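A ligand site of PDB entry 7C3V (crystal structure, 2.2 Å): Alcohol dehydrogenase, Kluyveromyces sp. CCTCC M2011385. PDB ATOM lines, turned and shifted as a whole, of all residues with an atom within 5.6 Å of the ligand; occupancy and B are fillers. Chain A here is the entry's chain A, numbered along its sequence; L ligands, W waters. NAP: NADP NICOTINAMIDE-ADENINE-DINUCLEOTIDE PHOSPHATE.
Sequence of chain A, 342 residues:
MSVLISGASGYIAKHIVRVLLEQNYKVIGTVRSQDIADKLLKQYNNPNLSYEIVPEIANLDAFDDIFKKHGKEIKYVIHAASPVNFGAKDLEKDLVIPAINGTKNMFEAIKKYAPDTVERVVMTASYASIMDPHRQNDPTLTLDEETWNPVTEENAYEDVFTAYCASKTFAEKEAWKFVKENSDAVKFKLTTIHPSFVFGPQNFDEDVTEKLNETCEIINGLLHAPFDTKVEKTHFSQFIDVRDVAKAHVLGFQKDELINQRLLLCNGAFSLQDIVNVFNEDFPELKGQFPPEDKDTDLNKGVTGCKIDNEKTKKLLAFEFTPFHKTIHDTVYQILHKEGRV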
ATOM      1  N   GLY A   7     -19.081 -15.682  14.018  1.00  0.00           N
ATOM      2  CA  GLY A   7     -20.147 -14.874  14.585  1.00  0.00           C
ATOM      3  C   GLY A   7     -20.054 -14.778  16.097  1.00  0.00           C
ATOM      4  O   GLY A   7     -21.017 -15.095  16.808  1.00  0.00           O
ATOM      5  N   ALA A   8     -18.903 -14.341  16.601  1.00  0.00           N
ATOM      6  CA  ALA A   8     -18.610 -14.407  18.030  1.00  0.00           C
ATOM      7  C   ALA A   8     -19.188 -13.246  18.821  1.00  0.00           C
ATOM      8  O   ALA A   8     -19.008 -13.212  20.048  1.00  0.00           O
ATOM      9  CB  ALA A   8     -17.098 -14.462  18.237  1.00  0.00           C
ATOM     10  N   SER A   9     -19.879 -12.304  18.186  1.00  0.00           N
ATOM     11  CA  SER A   9     -20.480 -11.184  18.897  1.00  0.00           C
ATOM     12  C   SER A   9     -21.964 -11.394  19.207  1.00  0.00           C
ATOM     13  O   SER A   9     -22.574 -10.533  19.842  1.00  0.00           O
ATOM     14  CB  SER A   9     -20.295  -9.889  18.094  1.00  0.00           C
ATOM     15  OG  SER A   9     -21.164  -9.852  16.980  1.00  0.00           O
ATOM     16  N   GLY A  10     -22.541 -12.508  18.788  1.00  0.00           N
ATOM     17  CA  GLY A  10     -23.956 -12.743  18.981  1.00  0.00           C
ATOM     18  C   GLY A  10     -24.310 -13.084  20.428  1.00  0.00           C
ATOM     19  O   GLY A  10     -23.466 -13.211  21.312  1.00  0.00           O
ATOM     20  N   TYR A  11     -25.613 -13.232  20.644  1.00  0.00           N
ATOM     21  CA  TYR A  11     -26.146 -13.519  21.973  1.00  0.00           C
ATOM     22  C   TYR A  11     -25.654 -14.859  22.489  1.00  0.00           C
ATOM     23  O   TYR A  11     -25.105 -14.942  23.599  1.00  0.00           O
ATOM     24  CB  TYR A  11     -27.671 -13.465  21.916  1.00  0.00           C
ATOM     25  CG  TYR A  11     -28.413 -14.080  23.086  1.00  0.00           C
ATOM     26  CD1 TYR A  11     -28.116 -13.731  24.395  1.00  0.00           C
ATOM     27  CD2 TYR A  11     -29.458 -14.983  22.874  1.00  0.00           C
ATOM     28  CE1 TYR A  11     -28.815 -14.276  25.457  1.00  0.00           C
ATOM     29  CE2 TYR A  11     -30.159 -15.521  23.915  1.00  0.00           C
ATOM     30  CZ  TYR A  11     -29.841 -15.172  25.213  1.00  0.00           C
ATOM     31  OH  TYR A  11     -30.548 -15.718  26.252  1.00  0.00           O
ATOM     32  N   ILE A  12     -25.822 -15.914  21.694  1.00  0.00           N
ATOM     33  CA  ILE A  12     -25.406 -17.249  22.122  1.00  0.00           C
ATOM     34  C   ILE A  12     -23.885 -17.362  22.115  1.00  0.00           C
ATOM     35  O   ILE A  12     -23.292 -17.950  23.037  1.00  0.00           O
ATOM     36  CB  ILE A  12     -26.055 -18.316  21.221  1.00  0.00           C
ATOM     37  CG1 ILE A  12     -27.567 -18.339  21.435  1.00  0.00           C
ATOM     38  CG2 ILE A  12     -25.444 -19.685  21.483  1.00  0.00           C
ATOM     39  CD1 ILE A  12     -28.328 -19.004  20.309  1.00  0.00           C
ATOM     40  N   ALA A  13     -23.229 -16.807  21.095  1.00  0.00           N
ATOM     41  CA  ALA A  13     -21.794 -17.014  20.954  1.00  0.00           C
ATOM     42  C   ALA A  13     -21.000 -16.344  22.066  1.00  0.00           C
ATOM     43  O   ALA A  13     -19.935 -16.832  22.448  1.00  0.00           O
ATOM     44  CB  ALA A  13     -21.321 -16.515  19.588  1.00  0.00           C
ATOM     45  N   ARG A  32     -17.803  -8.783  12.505  1.00  0.00           N
ATOM     46  CA  ARG A  32     -17.961  -8.051  11.250  1.00  0.00           C
ATOM     47  C   ARG A  32     -16.935  -6.921  11.124  1.00  0.00           C
ATOM     48  O   ARG A  32     -16.273  -6.792  10.082  1.00  0.00           O
ATOM     49  CB  ARG A  32     -19.383  -7.497  11.142  1.00  0.00           C
ATOM     50  CG  ARG A  32     -20.392  -8.468  10.576  1.00  0.00           C
ATOM     51  CD  ARG A  32     -21.516  -7.701   9.925  1.00  0.00           C
ATOM     52  NE  ARG A  32     -22.798  -8.386   9.944  1.00  0.00           N
ATOM     53  CZ  ARG A  32     -23.350  -8.973   8.889  1.00  0.00           C
ATOM     54  NH1 ARG A  32     -22.719  -8.957   7.722  1.00  0.00           N
ATOM     55  NH2 ARG A  32     -24.531  -9.564   8.996  1.00  0.00           N
ATOM     56  N   ILE A  36     -16.496  -3.605  16.811  1.00  0.00           N
ATOM     57  CA  ILE A  36     -17.075  -4.719  17.550  1.00  0.00           C
ATOM     58  C   ILE A  36     -15.978  -5.513  18.237  1.00  0.00           C
ATOM     59  O   ILE A  36     -16.076  -5.849  19.433  1.00  0.00           O
ATOM     60  CB  ILE A  36     -17.913  -5.605  16.621  1.00  0.00           C
ATOM     61  CG1 ILE A  36     -19.224  -4.901  16.238  1.00  0.00           C
ATOM     62  CG2 ILE A  36     -18.195  -6.965  17.260  1.00  0.00           C
ATOM     63  CD1 ILE A  36     -19.910  -5.499  15.024  1.00  0.00           C
ATOM     64  N   VAL A  54     -14.380 -10.873   9.737  1.00  0.00           N
ATOM     65  CA  VAL A  54     -15.124 -11.406   8.597  1.00  0.00           C
ATOM     66  C   VAL A  54     -16.415 -10.602   8.481  1.00  0.00           C
ATOM     67  O   VAL A  54     -17.374 -10.876   9.218  1.00  0.00           O
ATOM     68  CB  VAL A  54     -15.408 -12.915   8.745  1.00  0.00           C
ATOM     69  CG1 VAL A  54     -16.263 -13.408   7.586  1.00  0.00           C
ATOM     70  CG2 VAL A  54     -14.108 -13.684   8.801  1.00  0.00           C
ATOM     71  N   PRO A  55     -16.481  -9.619   7.592  1.00  0.00           N
ATOM     72  CA  PRO A  55     -17.629  -8.698   7.595  1.00  0.00           C
ATOM     73  C   PRO A  55     -18.909  -9.286   7.008  1.00  0.00           C
ATOM     74  O   PRO A  55     -19.981  -8.710   7.226  1.00  0.00           O
ATOM     75  CB  PRO A  55     -17.133  -7.510   6.766  1.00  0.00           C
ATOM     76  CG  PRO A  55     -16.067  -8.074   5.888  1.00  0.00           C
ATOM     77  CD  PRO A  55     -15.426  -9.191   6.656  1.00  0.00           C
ATOM     78  N   GLU A  56     -18.833 -10.391   6.272  1.00  0.00           N
ATOM     79  CA  GLU A  56     -20.026 -10.938   5.613  1.00  0.00           C
ATOM     80  C   GLU A  56     -19.755 -12.388   5.240  1.00  0.00           C
ATOM     81  O   GLU A  56     -18.912 -12.650   4.367  1.00  0.00           O
ATOM     82  CB  GLU A  56     -20.391 -10.094   4.398  1.00  0.00           C
ATOM     83  CG  GLU A  56     -21.614 -10.574   3.615  1.00  0.00           C
ATOM     84  CD  GLU A  56     -22.826 -10.818   4.507  1.00  0.00           C
ATOM     85  OE1 GLU A  56     -23.080 -12.004   4.827  1.00  0.00           O
ATOM     86  OE2 GLU A  56     -23.511  -9.844   4.875  1.00  0.00           O
ATOM     87  N   ILE A  57     -20.467 -13.309   5.876  1.00  0.00           N
ATOM     88  CA  ILE A  57     -20.242 -14.728   5.627  1.00  0.00           C
ATOM     89  C   ILE A  57     -20.801 -15.189   4.293  1.00  0.00           C
ATOM     90  O   ILE A  57     -20.366 -16.226   3.766  1.00  0.00           O
ATOM     91  CB  ILE A  57     -20.830 -15.574   6.772  1.00  0.00           C
ATOM     92  CG1 ILE A  57     -22.345 -15.348   6.877  1.00  0.00           C
ATOM     93  CG2 ILE A  57     -20.153 -15.240   8.091  1.00  0.00           C
ATOM     94  CD1 ILE A  57     -23.007 -16.130   7.999  1.00  0.00           C
ATOM     95  N   ALA A  58     -21.755 -14.459   3.723  1.00  0.00           N
ATOM     96  CA  ALA A  58     -22.379 -14.875   2.466  1.00  0.00           C
ATOM     97  C   ALA A  58     -21.453 -14.760   1.273  1.00  0.00           C
ATOM     98  O   ALA A  58     -21.840 -15.153   0.168  1.00  0.00           O
ATOM     99  CB  ALA A  58     -23.646 -14.054   2.204  1.00  0.00           C
ATOM    100  N   ALA A  80     -21.158 -20.726  14.312  1.00  0.00           N
ATOM    101  CA  ALA A  80     -22.377 -20.174  14.883  1.00  0.00           C
ATOM    102  C   ALA A  80     -22.903 -18.957  14.132  1.00  0.00           C
ATOM    103  O   ALA A  80     -23.971 -18.445  14.491  1.00  0.00           O
ATOM    104  CB  ALA A  80     -22.134 -19.798  16.356  1.00  0.00           C
ATOM    105  N   ALA A  81     -22.205 -18.499  13.105  1.00  0.00           N
ATOM    106  CA  ALA A  81     -22.608 -17.295  12.385  1.00  0.00           C
ATOM    107  C   ALA A  81     -23.777 -17.610  11.447  1.00  0.00           C
ATOM    108  O   ALA A  81     -23.638 -18.389  10.500  1.00  0.00           O
ATOM    109  CB  ALA A  81     -21.434 -16.721  11.588  1.00  0.00           C
ATOM    110  N   SER A  82     -24.927 -16.999  11.718  1.00  0.00           N
ATOM    111  CA  SER A  82     -26.116 -17.106  10.889  1.00  0.00           C
ATOM    112  C   SER A  82     -27.101 -16.018  11.323  1.00  0.00           C
ATOM    113  O   SER A  82     -27.164 -15.693  12.505  1.00  0.00           O
ATOM    114  CB  SER A  82     -26.751 -18.488  11.006  1.00  0.00           C
ATOM    115  OG  SER A  82     -27.590 -18.774   9.898  1.00  0.00           O
ATOM    116  N   PRO A  83     -27.859 -15.430  10.397  1.00  0.00           N
ATOM    117  CA  PRO A  83     -28.695 -14.272  10.759  1.00  0.00           C
ATOM    118  C   PRO A  83     -29.994 -14.692  11.436  1.00  0.00           C
ATOM    119  O   PRO A  83     -30.706 -15.586  10.973  1.00  0.00           O
ATOM    120  CB  PRO A  83     -28.968 -13.607   9.402  1.00  0.00           C
ATOM    121  CG  PRO A  83     -28.834 -14.705   8.403  1.00  0.00           C
ATOM    122  CD  PRO A  83     -27.794 -15.650   8.942  1.00  0.00           C
ATOM    123  N   VAL A  84     -30.303 -14.016  12.549  1.00  0.00           N
ATOM    124  CA  VAL A  84     -31.571 -14.157  13.251  1.00  0.00           C
ATOM    125  C   VAL A  84     -32.242 -12.793  13.201  1.00  0.00           C
ATOM    126  O   VAL A  84     -32.060 -11.954  14.095  1.00  0.00           O
ATOM    127  CB  VAL A  84     -31.399 -14.638  14.705  1.00  0.00           C
ATOM    128  CG1 VAL A  84     -32.761 -14.776  15.380  1.00  0.00           C
ATOM    129  CG2 VAL A  84     -30.650 -15.942  14.740  1.00  0.00           C
ATOM    130  N   PRO A  98     -27.069 -15.947   3.312  1.00  0.00           N
ATOM    131  CA  PRO A  98     -25.971 -15.962   4.293  1.00  0.00           C
ATOM    132  C   PRO A  98     -25.889 -17.256   5.084  1.00  0.00           C
ATOM    133  O   PRO A  98     -24.785 -17.706   5.405  1.00  0.00           O
ATOM    134  CB  PRO A  98     -26.278 -14.761   5.215  1.00  0.00           C
ATOM    135  CG  PRO A  98     -27.305 -13.976   4.498  1.00  0.00           C
ATOM    136  CD  PRO A  98     -28.079 -14.937   3.668  1.00  0.00           C
ATOM    137  N   THR A 124     -24.002 -24.525  14.765  1.00  0.00           N
ATOM    138  CA  THR A 124     -25.237 -24.094  15.408  1.00  0.00           C
ATOM    139  C   THR A 124     -26.345 -24.136  14.369  1.00  0.00           C
ATOM    140  O   THR A 124     -26.531 -23.203  13.590  1.00  0.00           O
ATOM    141  CB  THR A 124     -25.105 -22.689  15.995  1.00  0.00           C
ATOM    142  OG1 THR A 124     -23.860 -22.579  16.692  1.00  0.00           O
ATOM    143  CG2 THR A 124     -26.250 -22.434  16.960  1.00  0.00           C
ATOM    144  N   ALA A 125     -27.094 -25.240  14.351  1.00  0.00           N
ATOM    145  CA  ALA A 125     -28.298 -25.317  13.550  1.00  0.00           C
ATOM    146  C   ALA A 125     -29.437 -24.718  14.358  1.00  0.00           C
ATOM    147  O   ALA A 125     -29.264 -23.682  15.007  1.00  0.00           O
ATOM    148  CB  ALA A 125     -28.596 -26.752  13.136  1.00  0.00           C
ATOM    149  N   SER A 126     -30.600 -25.366  14.325  1.00  0.00           N
ATOM    150  CA  SER A 126     -31.727 -24.872  15.098  1.00  0.00           C
ATOM    151  C   SER A 126     -32.754 -25.973  15.269  1.00  0.00           C
ATOM    152  O   SER A 126     -32.838 -26.894  14.452  1.00  0.00           O
ATOM    153  CB  SER A 126     -32.364 -23.643  14.441  1.00  0.00           C
ATOM    154  OG  SER A 126     -33.537 -23.250  15.145  1.00  0.00           O
ATOM    155  N   TYR A 127     -33.530 -25.867  16.345  1.00  0.00           N
ATOM    156  CA  TYR A 127     -34.774 -26.614  16.447  1.00  0.00           C
ATOM    157  C   TYR A 127     -35.624 -26.393  15.208  1.00  0.00           C
ATOM    158  O   TYR A 127     -36.357 -27.294  14.791  1.00  0.00           O
ATOM    159  CB  TYR A 127     -35.497 -26.173  17.731  1.00  0.00           C
ATOM    160  CG  TYR A 127     -36.978 -26.455  17.848  1.00  0.00           C
ATOM    161  CD1 TYR A 127     -37.457 -27.741  18.077  1.00  0.00           C
ATOM    162  CD2 TYR A 127     -37.900 -25.412  17.798  1.00  0.00           C
ATOM    163  CE1 TYR A 127     -38.816 -27.982  18.222  1.00  0.00           C
ATOM    164  CE2 TYR A 127     -39.264 -25.649  17.935  1.00  0.00           C
ATOM    165  CZ  TYR A 127     -39.717 -26.938  18.148  1.00  0.00           C
ATOM    166  OH  TYR A 127     -41.063 -27.175  18.289  1.00  0.00           O
ATOM    167  N   TYR A 164     -36.727 -17.954   7.884  1.00  0.00           N
ATOM    168  CA  TYR A 164     -35.630 -18.201   8.815  1.00  0.00           C
ATOM    169  C   TYR A 164     -35.456 -19.693   9.072  1.00  0.00           C
ATOM    170  O   TYR A 164     -34.333 -20.200   9.094  1.00  0.00           O
ATOM    171  CB  TYR A 164     -35.850 -17.463  10.133  1.00  0.00           C
ATOM    172  CG  TYR A 164     -34.914 -17.943  11.207  1.00  0.00           C
ATOM    173  CD1 TYR A 164     -33.549 -17.660  11.139  1.00  0.00           C
ATOM    174  CD2 TYR A 164     -35.358 -18.713  12.272  1.00  0.00           C
ATOM    175  CE1 TYR A 164     -32.677 -18.101  12.101  1.00  0.00           C
ATOM    176  CE2 TYR A 164     -34.487 -19.167  13.240  1.00  0.00           C
ATOM    177  CZ  TYR A 164     -33.146 -18.860  13.148  1.00  0.00           C
ATOM    178  OH  TYR A 164     -32.269 -19.307  14.118  1.00  0.00           O
ATOM    179  N   LYS A 168     -32.141 -22.111   8.178  1.00  0.00           N
ATOM    180  CA  LYS A 168     -31.487 -23.072   9.057  1.00  0.00           C
ATOM    181  C   LYS A 168     -31.535 -24.483   8.487  1.00  0.00           C
ATOM    182  O   LYS A 168     -30.543 -25.223   8.556  1.00  0.00           O
ATOM    183  CB  LYS A 168     -32.123 -23.036  10.446  1.00  0.00           C
ATOM    184  CG  LYS A 168     -32.161 -21.651  11.083  1.00  0.00           C
ATOM    185  CD  LYS A 168     -30.754 -21.112  11.308  1.00  0.00           C
ATOM    186  CE  LYS A 168     -29.908 -22.086  12.101  1.00  0.00           C
ATOM    187  NZ  LYS A 168     -28.552 -21.545  12.381  1.00  0.00           N
ATOM    188  N   HIS A 194     -29.183 -27.879  18.022  1.00  0.00           N
ATOM    189  CA  HIS A 194     -30.509 -27.466  17.559  1.00  0.00           C
ATOM    190  C   HIS A 194     -31.284 -26.838  18.719  1.00  0.00           C
ATOM    191  O   HIS A 194     -32.178 -27.473  19.300  1.00  0.00           O
ATOM    192  CB  HIS A 194     -31.282 -28.645  16.979  1.00  0.00           C
ATOM    193  CG  HIS A 194     -30.631 -29.273  15.794  1.00  0.00           C
ATOM    194  ND1 HIS A 194     -31.135 -29.159  14.522  1.00  0.00           N
ATOM    195  CD2 HIS A 194     -29.512 -30.030  15.691  1.00  0.00           C
ATOM    196  CE1 HIS A 194     -30.353 -29.819  13.679  1.00  0.00           C
ATOM    197  NE2 HIS A 194     -29.361 -30.349  14.361  1.00  0.00           N
ATOM    198  N   PRO A 195     -30.987 -25.593  19.072  1.00  0.00           N
ATOM    199  CA  PRO A 195     -31.741 -24.932  20.137  1.00  0.00           C
ATOM    200  C   PRO A 195     -33.093 -24.429  19.655  1.00  0.00           C
ATOM    201  O   PRO A 195     -33.276 -24.087  18.483  1.00  0.00           O
ATOM    202  CB  PRO A 195     -30.839 -23.758  20.541  1.00  0.00           C
ATOM    203  CG  PRO A 195     -29.534 -23.941  19.774  1.00  0.00           C
ATOM    204  CD  PRO A 195     -29.893 -24.745  18.565  1.00  0.00           C
ATOM    205  N   SER A 196     -34.048 -24.389  20.573  1.00  0.00           N
ATOM    206  CA  SER A 196     -35.333 -23.747  20.306  1.00  0.00           C
ATOM    207  C   SER A 196     -35.214 -22.272  20.658  1.00  0.00           C
ATOM    208  O   SER A 196     -34.122 -21.695  20.576  1.00  0.00           O
ATOM    209  CB  SER A 196     -36.468 -24.422  21.080  1.00  0.00           C
ATOM    210  OG  SER A 196     -36.064 -24.789  22.382  1.00  0.00           O
ATOM    211  N   PHE A 197     -36.319 -21.639  21.063  1.00  0.00           N
ATOM    212  CA  PHE A 197     -36.254 -20.228  21.427  1.00  0.00           C
ATOM    213  C   PHE A 197     -35.326 -20.034  22.624  1.00  0.00           C
ATOM    214  O   PHE A 197     -35.634 -20.483  23.739  1.00  0.00           O
ATOM    215  CB  PHE A 197     -37.646 -19.677  21.709  1.00  0.00           C
ATOM    216  CG  PHE A 197     -38.398 -19.288  20.477  1.00  0.00           C
ATOM    217  CD1 PHE A 197     -38.353 -17.991  20.001  1.00  0.00           C
ATOM    218  CD2 PHE A 197     -39.137 -20.231  19.772  1.00  0.00           C
ATOM    219  CE1 PHE A 197     -39.043 -17.635  18.858  1.00  0.00           C
ATOM    220  CE2 PHE A 197     -39.825 -19.886  18.621  1.00  0.00           C
ATOM    221  CZ  PHE A 197     -39.777 -18.582  18.161  1.00  0.00           C
ATOM    222  N   VAL A 198     -34.195 -19.388  22.397  1.00  0.00           N
ATOM    223  CA  VAL A 198     -33.145 -19.278  23.394  1.00  0.00           C
ATOM    224  C   VAL A 198     -33.415 -18.053  24.260  1.00  0.00           C
ATOM    225  O   VAL A 198     -33.412 -16.924  23.761  1.00  0.00           O
ATOM    226  CB  VAL A 198     -31.762 -19.202  22.747  1.00  0.00           C
ATOM    227  CG1 VAL A 198     -30.695 -19.040  23.795  1.00  0.00           C
ATOM    228  CG2 VAL A 198     -31.497 -20.459  21.927  1.00  0.00           C
ATOM    229  N   ASN A 213     -31.309  -8.934  21.246  1.00  0.00           N
ATOM    230  CA  ASN A 213     -31.402  -9.928  20.175  1.00  0.00           C
ATOM    231  C   ASN A 213     -32.839 -10.400  20.037  1.00  0.00           C
ATOM    232  O   ASN A 213     -33.661 -10.253  20.941  1.00  0.00           O
ATOM    233  CB  ASN A 213     -30.466 -11.100  20.447  1.00  0.00           C
ATOM    234  CG  ASN A 213     -30.857 -11.878  21.689  1.00  0.00           C
ATOM    235  OD1 ASN A 213     -30.532 -11.492  22.810  1.00  0.00           O
ATOM    236  ND2 ASN A 213     -31.553 -12.992  21.491  1.00  0.00           N
ATOM    237  N   THR A 215     -34.800 -13.219  19.960  1.00  0.00           N
ATOM    238  CA  THR A 215     -35.581 -14.060  20.856  1.00  0.00           C
ATOM    239  C   THR A 215     -35.688 -13.441  22.244  1.00  0.00           C
ATOM    240  O   THR A 215     -36.758 -13.497  22.870  1.00  0.00           O
ATOM    241  CB  THR A 215     -34.978 -15.468  20.939  1.00  0.00           C
ATOM    242  OG1 THR A 215     -33.596 -15.399  21.312  1.00  0.00           O
ATOM    243  CG2 THR A 215     -35.094 -16.154  19.586  1.00  0.00           C
HETATM  244  PA  NAP L   1     -27.553 -12.983  17.247  1.00  0.00           P
HETATM  245  O1A NAP L   1     -28.172 -12.033  16.250  1.00  0.00           O
HETATM  246  O2A NAP L   1     -27.431 -12.569  18.691  1.00  0.00           O
HETATM  247  O5B NAP L   1     -26.091 -13.429  16.735  1.00  0.00           O
HETATM  248  C5B NAP L   1     -25.821 -13.742  15.371  1.00  0.00           C
HETATM  249  C4B NAP L   1     -24.311 -13.665  15.154  1.00  0.00           C
HETATM  250  O4B NAP L   1     -23.992 -14.060  13.815  1.00  0.00           O
HETATM  251  C3B NAP L   1     -23.865 -12.214  15.302  1.00  0.00           C
HETATM  252  O3B NAP L   1     -22.531 -12.193  15.813  1.00  0.00           O
HETATM  253  C2B NAP L   1     -23.853 -11.716  13.879  1.00  0.00           C
HETATM  254  O2B NAP L   1     -22.969 -10.626  13.685  1.00  0.00           O
HETATM  255  C1B NAP L   1     -23.431 -12.953  13.108  1.00  0.00           C
HETATM  256  N9A NAP L   1     -23.944 -12.881  11.721  1.00  0.00           N
HETATM  257  C8A NAP L   1     -25.226 -13.054  11.345  1.00  0.00           C
HETATM  258  N7A NAP L   1     -25.353 -12.906  10.000  1.00  0.00           N
HETATM  259  C5A NAP L   1     -24.142 -12.632   9.509  1.00  0.00           C
HETATM  260  C6A NAP L   1     -23.570 -12.357   8.165  1.00  0.00           C
HETATM  261  N6A NAP L   1     -24.362 -12.358   7.063  1.00  0.00           N
HETATM  262  N1A NAP L   1     -22.246 -12.116   8.078  1.00  0.00           N
HETATM  263  C2A NAP L   1     -21.458 -12.110   9.172  1.00  0.00           C
HETATM  264  N3A NAP L   1     -21.902 -12.345  10.423  1.00  0.00           N
HETATM  265  C4A NAP L   1     -23.214 -12.604  10.648  1.00  0.00           C
HETATM  266  O3  NAP L   1     -28.358 -14.372  17.147  1.00  0.00           O
HETATM  267  PN  NAP L   1     -28.326 -15.517  18.275  1.00  0.00           P
HETATM  268  O1N NAP L   1     -29.699 -15.596  18.903  1.00  0.00           O
HETATM  269  O2N NAP L   1     -27.077 -15.398  19.132  1.00  0.00           O
HETATM  270  O5D NAP L   1     -28.111 -16.810  17.341  1.00  0.00           O
HETATM  271  C5D NAP L   1     -26.807 -17.349  17.180  1.00  0.00           C
HETATM  272  C4D NAP L   1     -26.916 -18.620  16.341  1.00  0.00           C
HETATM  273  O4D NAP L   1     -27.760 -19.539  17.022  1.00  0.00           O
HETATM  274  C3D NAP L   1     -27.540 -18.365  14.978  1.00  0.00           C
HETATM  275  O3D NAP L   1     -26.813 -19.122  14.022  1.00  0.00           O
HETATM  276  C2D NAP L   1     -28.937 -18.940  15.078  1.00  0.00           C
HETATM  277  O2D NAP L   1     -29.371 -19.482  13.834  1.00  0.00           O
HETATM  278  C1D NAP L   1     -28.769 -20.019  16.138  1.00  0.00           C
HETATM  279  N1N NAP L   1     -30.019 -20.269  16.862  1.00  0.00           N
HETATM  280  C2N NAP L   1     -30.580 -19.307  17.617  1.00  0.00           C
HETATM  281  C3N NAP L   1     -31.765 -19.586  18.301  1.00  0.00           C
HETATM  282  C7N NAP L   1     -32.430 -18.555  19.157  1.00  0.00           C
HETATM  283  O7N NAP L   1     -33.503 -18.837  19.661  1.00  0.00           O
HETATM  284  N7N NAP L   1     -31.840 -17.370  19.354  1.00  0.00           N
HETATM  285  C4N NAP L   1     -32.341 -20.841  18.195  1.00  0.00           C
HETATM  286  C5N NAP L   1     -31.728 -21.800  17.415  1.00  0.00           C
HETATM  287  C6N NAP L   1     -30.555 -21.489  16.746  1.00  0.00           C
HETATM  288  P2B NAP L   1     -23.561  -9.134  13.547  1.00  0.00           P
HETATM  289  O1X NAP L   1     -22.330  -8.249  13.556  1.00  0.00           O
HETATM  290  O2X NAP L   1     -24.303  -9.174  12.234  1.00  0.00           O
HETATM  291  O3X NAP L   1     -24.464  -8.960  14.749  1.00  0.00           O
HETATM  292  O   HOH W   1     -19.895 -11.960  12.616  1.00  0.00           O
HETATM  293  O   HOH W   2     -22.941  -5.543  12.698  1.00  0.00           O
HETATM  294  O   HOH W   3     -20.043  -9.549  14.258  1.00  0.00           O
HETATM  295  O   HOH W   4     -24.392 -15.891  18.712  1.00  0.00           O
HETATM  296  O   HOH W   5     -24.597 -21.287  12.596  1.00  0.00           O
HETATM  297  O   HOH W   6     -27.439 -10.546   9.239  1.00  0.00           O
HETATM  298  O   HOH W   7     -31.080 -11.899  16.630  1.00  0.00           O
HETATM  299  O   HOH W   8     -23.292 -16.560  16.274  1.00  0.00           O
HETATM  300  O   HOH W   9     -28.597 -11.909  13.590  1.00  0.00           O
HETATM  301  O   HOH W  10     -27.002 -10.052  19.648  1.00  0.00           O
HETATM  302  O   HOH W  11     -31.692 -14.077  18.795  1.00  0.00           O
HETATM  303  O   HOH W  12     -27.190 -10.329  12.220  1.00  0.00           O
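The side-chain hydroxyl of Ser 9 is in hydrogen-bond range of an oxygen (O3B) of the ligand. The side-chain hydroxyl (OH) of Tyr 164 sits at hydrogen-bond distance from an oxygen (O2D) of the ligand (2.9 Å). An oxygen (O2X) of the ligand is in salt-bridge range of the guanidinium group (NE) of Arg 32 (2.9 Å). The backbone NH (N) of Ile 12 sits at hydrogen-bond distance from an oxygen (O2N) of the ligand (2.9 Å). An oxygen (O7N) of the ligand lies within hydrogen-bond range of the backbone NH (N) of Val 198, 2.9 Å away. The backbone carbonyl oxygen of Ala 80 sits at hydrogen-bond distance from an oxygen (O3D) of the ligand (3.0 Å). An oxygen (O3B) of the ligand lies within hydrogen-bond range of the backbone carbonyl oxygen (O) of Gly 7. O2D of the ligand lies within hydrogen-bond range of NZ of Lys 168 (2.7 Å). The backbone NH of Gly 10 sits at hydrogen-bond distance from an oxygen (O3B) of the ligand, at 3.0 Å. N of Tyr 11 sits at hydrogen-bond distance from O2A of the ligand (2.7 Å). N1A of the ligand sits at hydrogen-bond distance from N of Ile 57, at 3.1 Å. The side-chain carboxylate of Glu 56 sits at hydrogen-bond distance from a nitrogen (N6A) of the ligand (2.6 Å). The side-chain hydroxyl (OG1) of Thr 215 is in hydrogen-bond range of a nitrogen (N7N) of the ligand (3.3 Å).
The side-chain hydroxyl (OG) of Ser 126 is in hydrogen-bond range of the backbone carbonyl oxygen (O) of Pro 195. The side-chain hydroxyl of Thr 215 is in hydrogen-bond range of the backbone carbonyl oxygen of Val 198 (2.9 Å). The side-chain carboxylate of Glu 56 sits at hydrogen-bond distance from the backbone NH of Ala 58 (3.0 Å). The backbone NH (N) of Tyr 127 sits at hydrogen-bond distance from the backbone carbonyl oxygen (O) of Pro 195 (2.8 Å). The backbone carbonyl oxygen (O) of Ser 126 sits at hydrogen-bond distance from a ring nitrogen (ND1) of His 194, at 2.8 Å. The side-chain hydroxyl of Thr 215 is in hydrogen-bond range of the side-chain amide nitrogen of Asn 213 (3.2 Å). The side-chain amino group (NZ) of Lys 168 sits close to the backbone carbonyl oxygen (O) of Ala 125 (3.5 Å). The side-chain carboxylate (OE2) of Glu 56 is in salt-bridge range of the guanidinium group (NH1) of Arg 32, 3.1 Å away.
The backbone carbonyl oxygen (O) of Ser 196 lies close to an oxygen (O7N) of the ligand (3.1 Å). Residues that only touch the ligand: Pro 195, Ala 125, Ser 82, Ser 126, Thr 124, Val 84, Phe 197, Pro 83, Pro 98, Ala 81, Asn 213 and Ile 36. Hydrophobic or aromatic side chains that line the ligand: Tyr 11, Ile 12, Ile 36, Ile 57, Pro 83, Val 84, Pro 98, Tyr 164, Pro 195 and Val 198. The nearest printed residue that does not touch the ligand is Pro 55 (4.2 Å).
Water W9 lies within hydrogen-bond range of O1A of the ligand (2.7 Å) and N of Val 84 (2.9 Å). Water W4 lies within hydrogen-bond range of O2N of the ligand (2.8 Å), N of Ala 13 (2.8 Å) and N of Ile 12 (3.3 Å). Water W7 bridges O of Val 84 (2.7 Å) and O1A of the ligand (2.9 Å). Water W6 lies within hydrogen-bond range of NH2 of Arg 32 and N7A of the ligand. Water W8 bridges O of Ala 80 and O of Gly 7. Water W5 lies within hydrogen-bond range of the backbone carbonyl oxygen (O) of Thr 124 (2.9 Å), an oxygen (O3D) of the ligand (3.4 Å) and the backbone carbonyl oxygen (O) of Ala 80 (3.5 Å).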
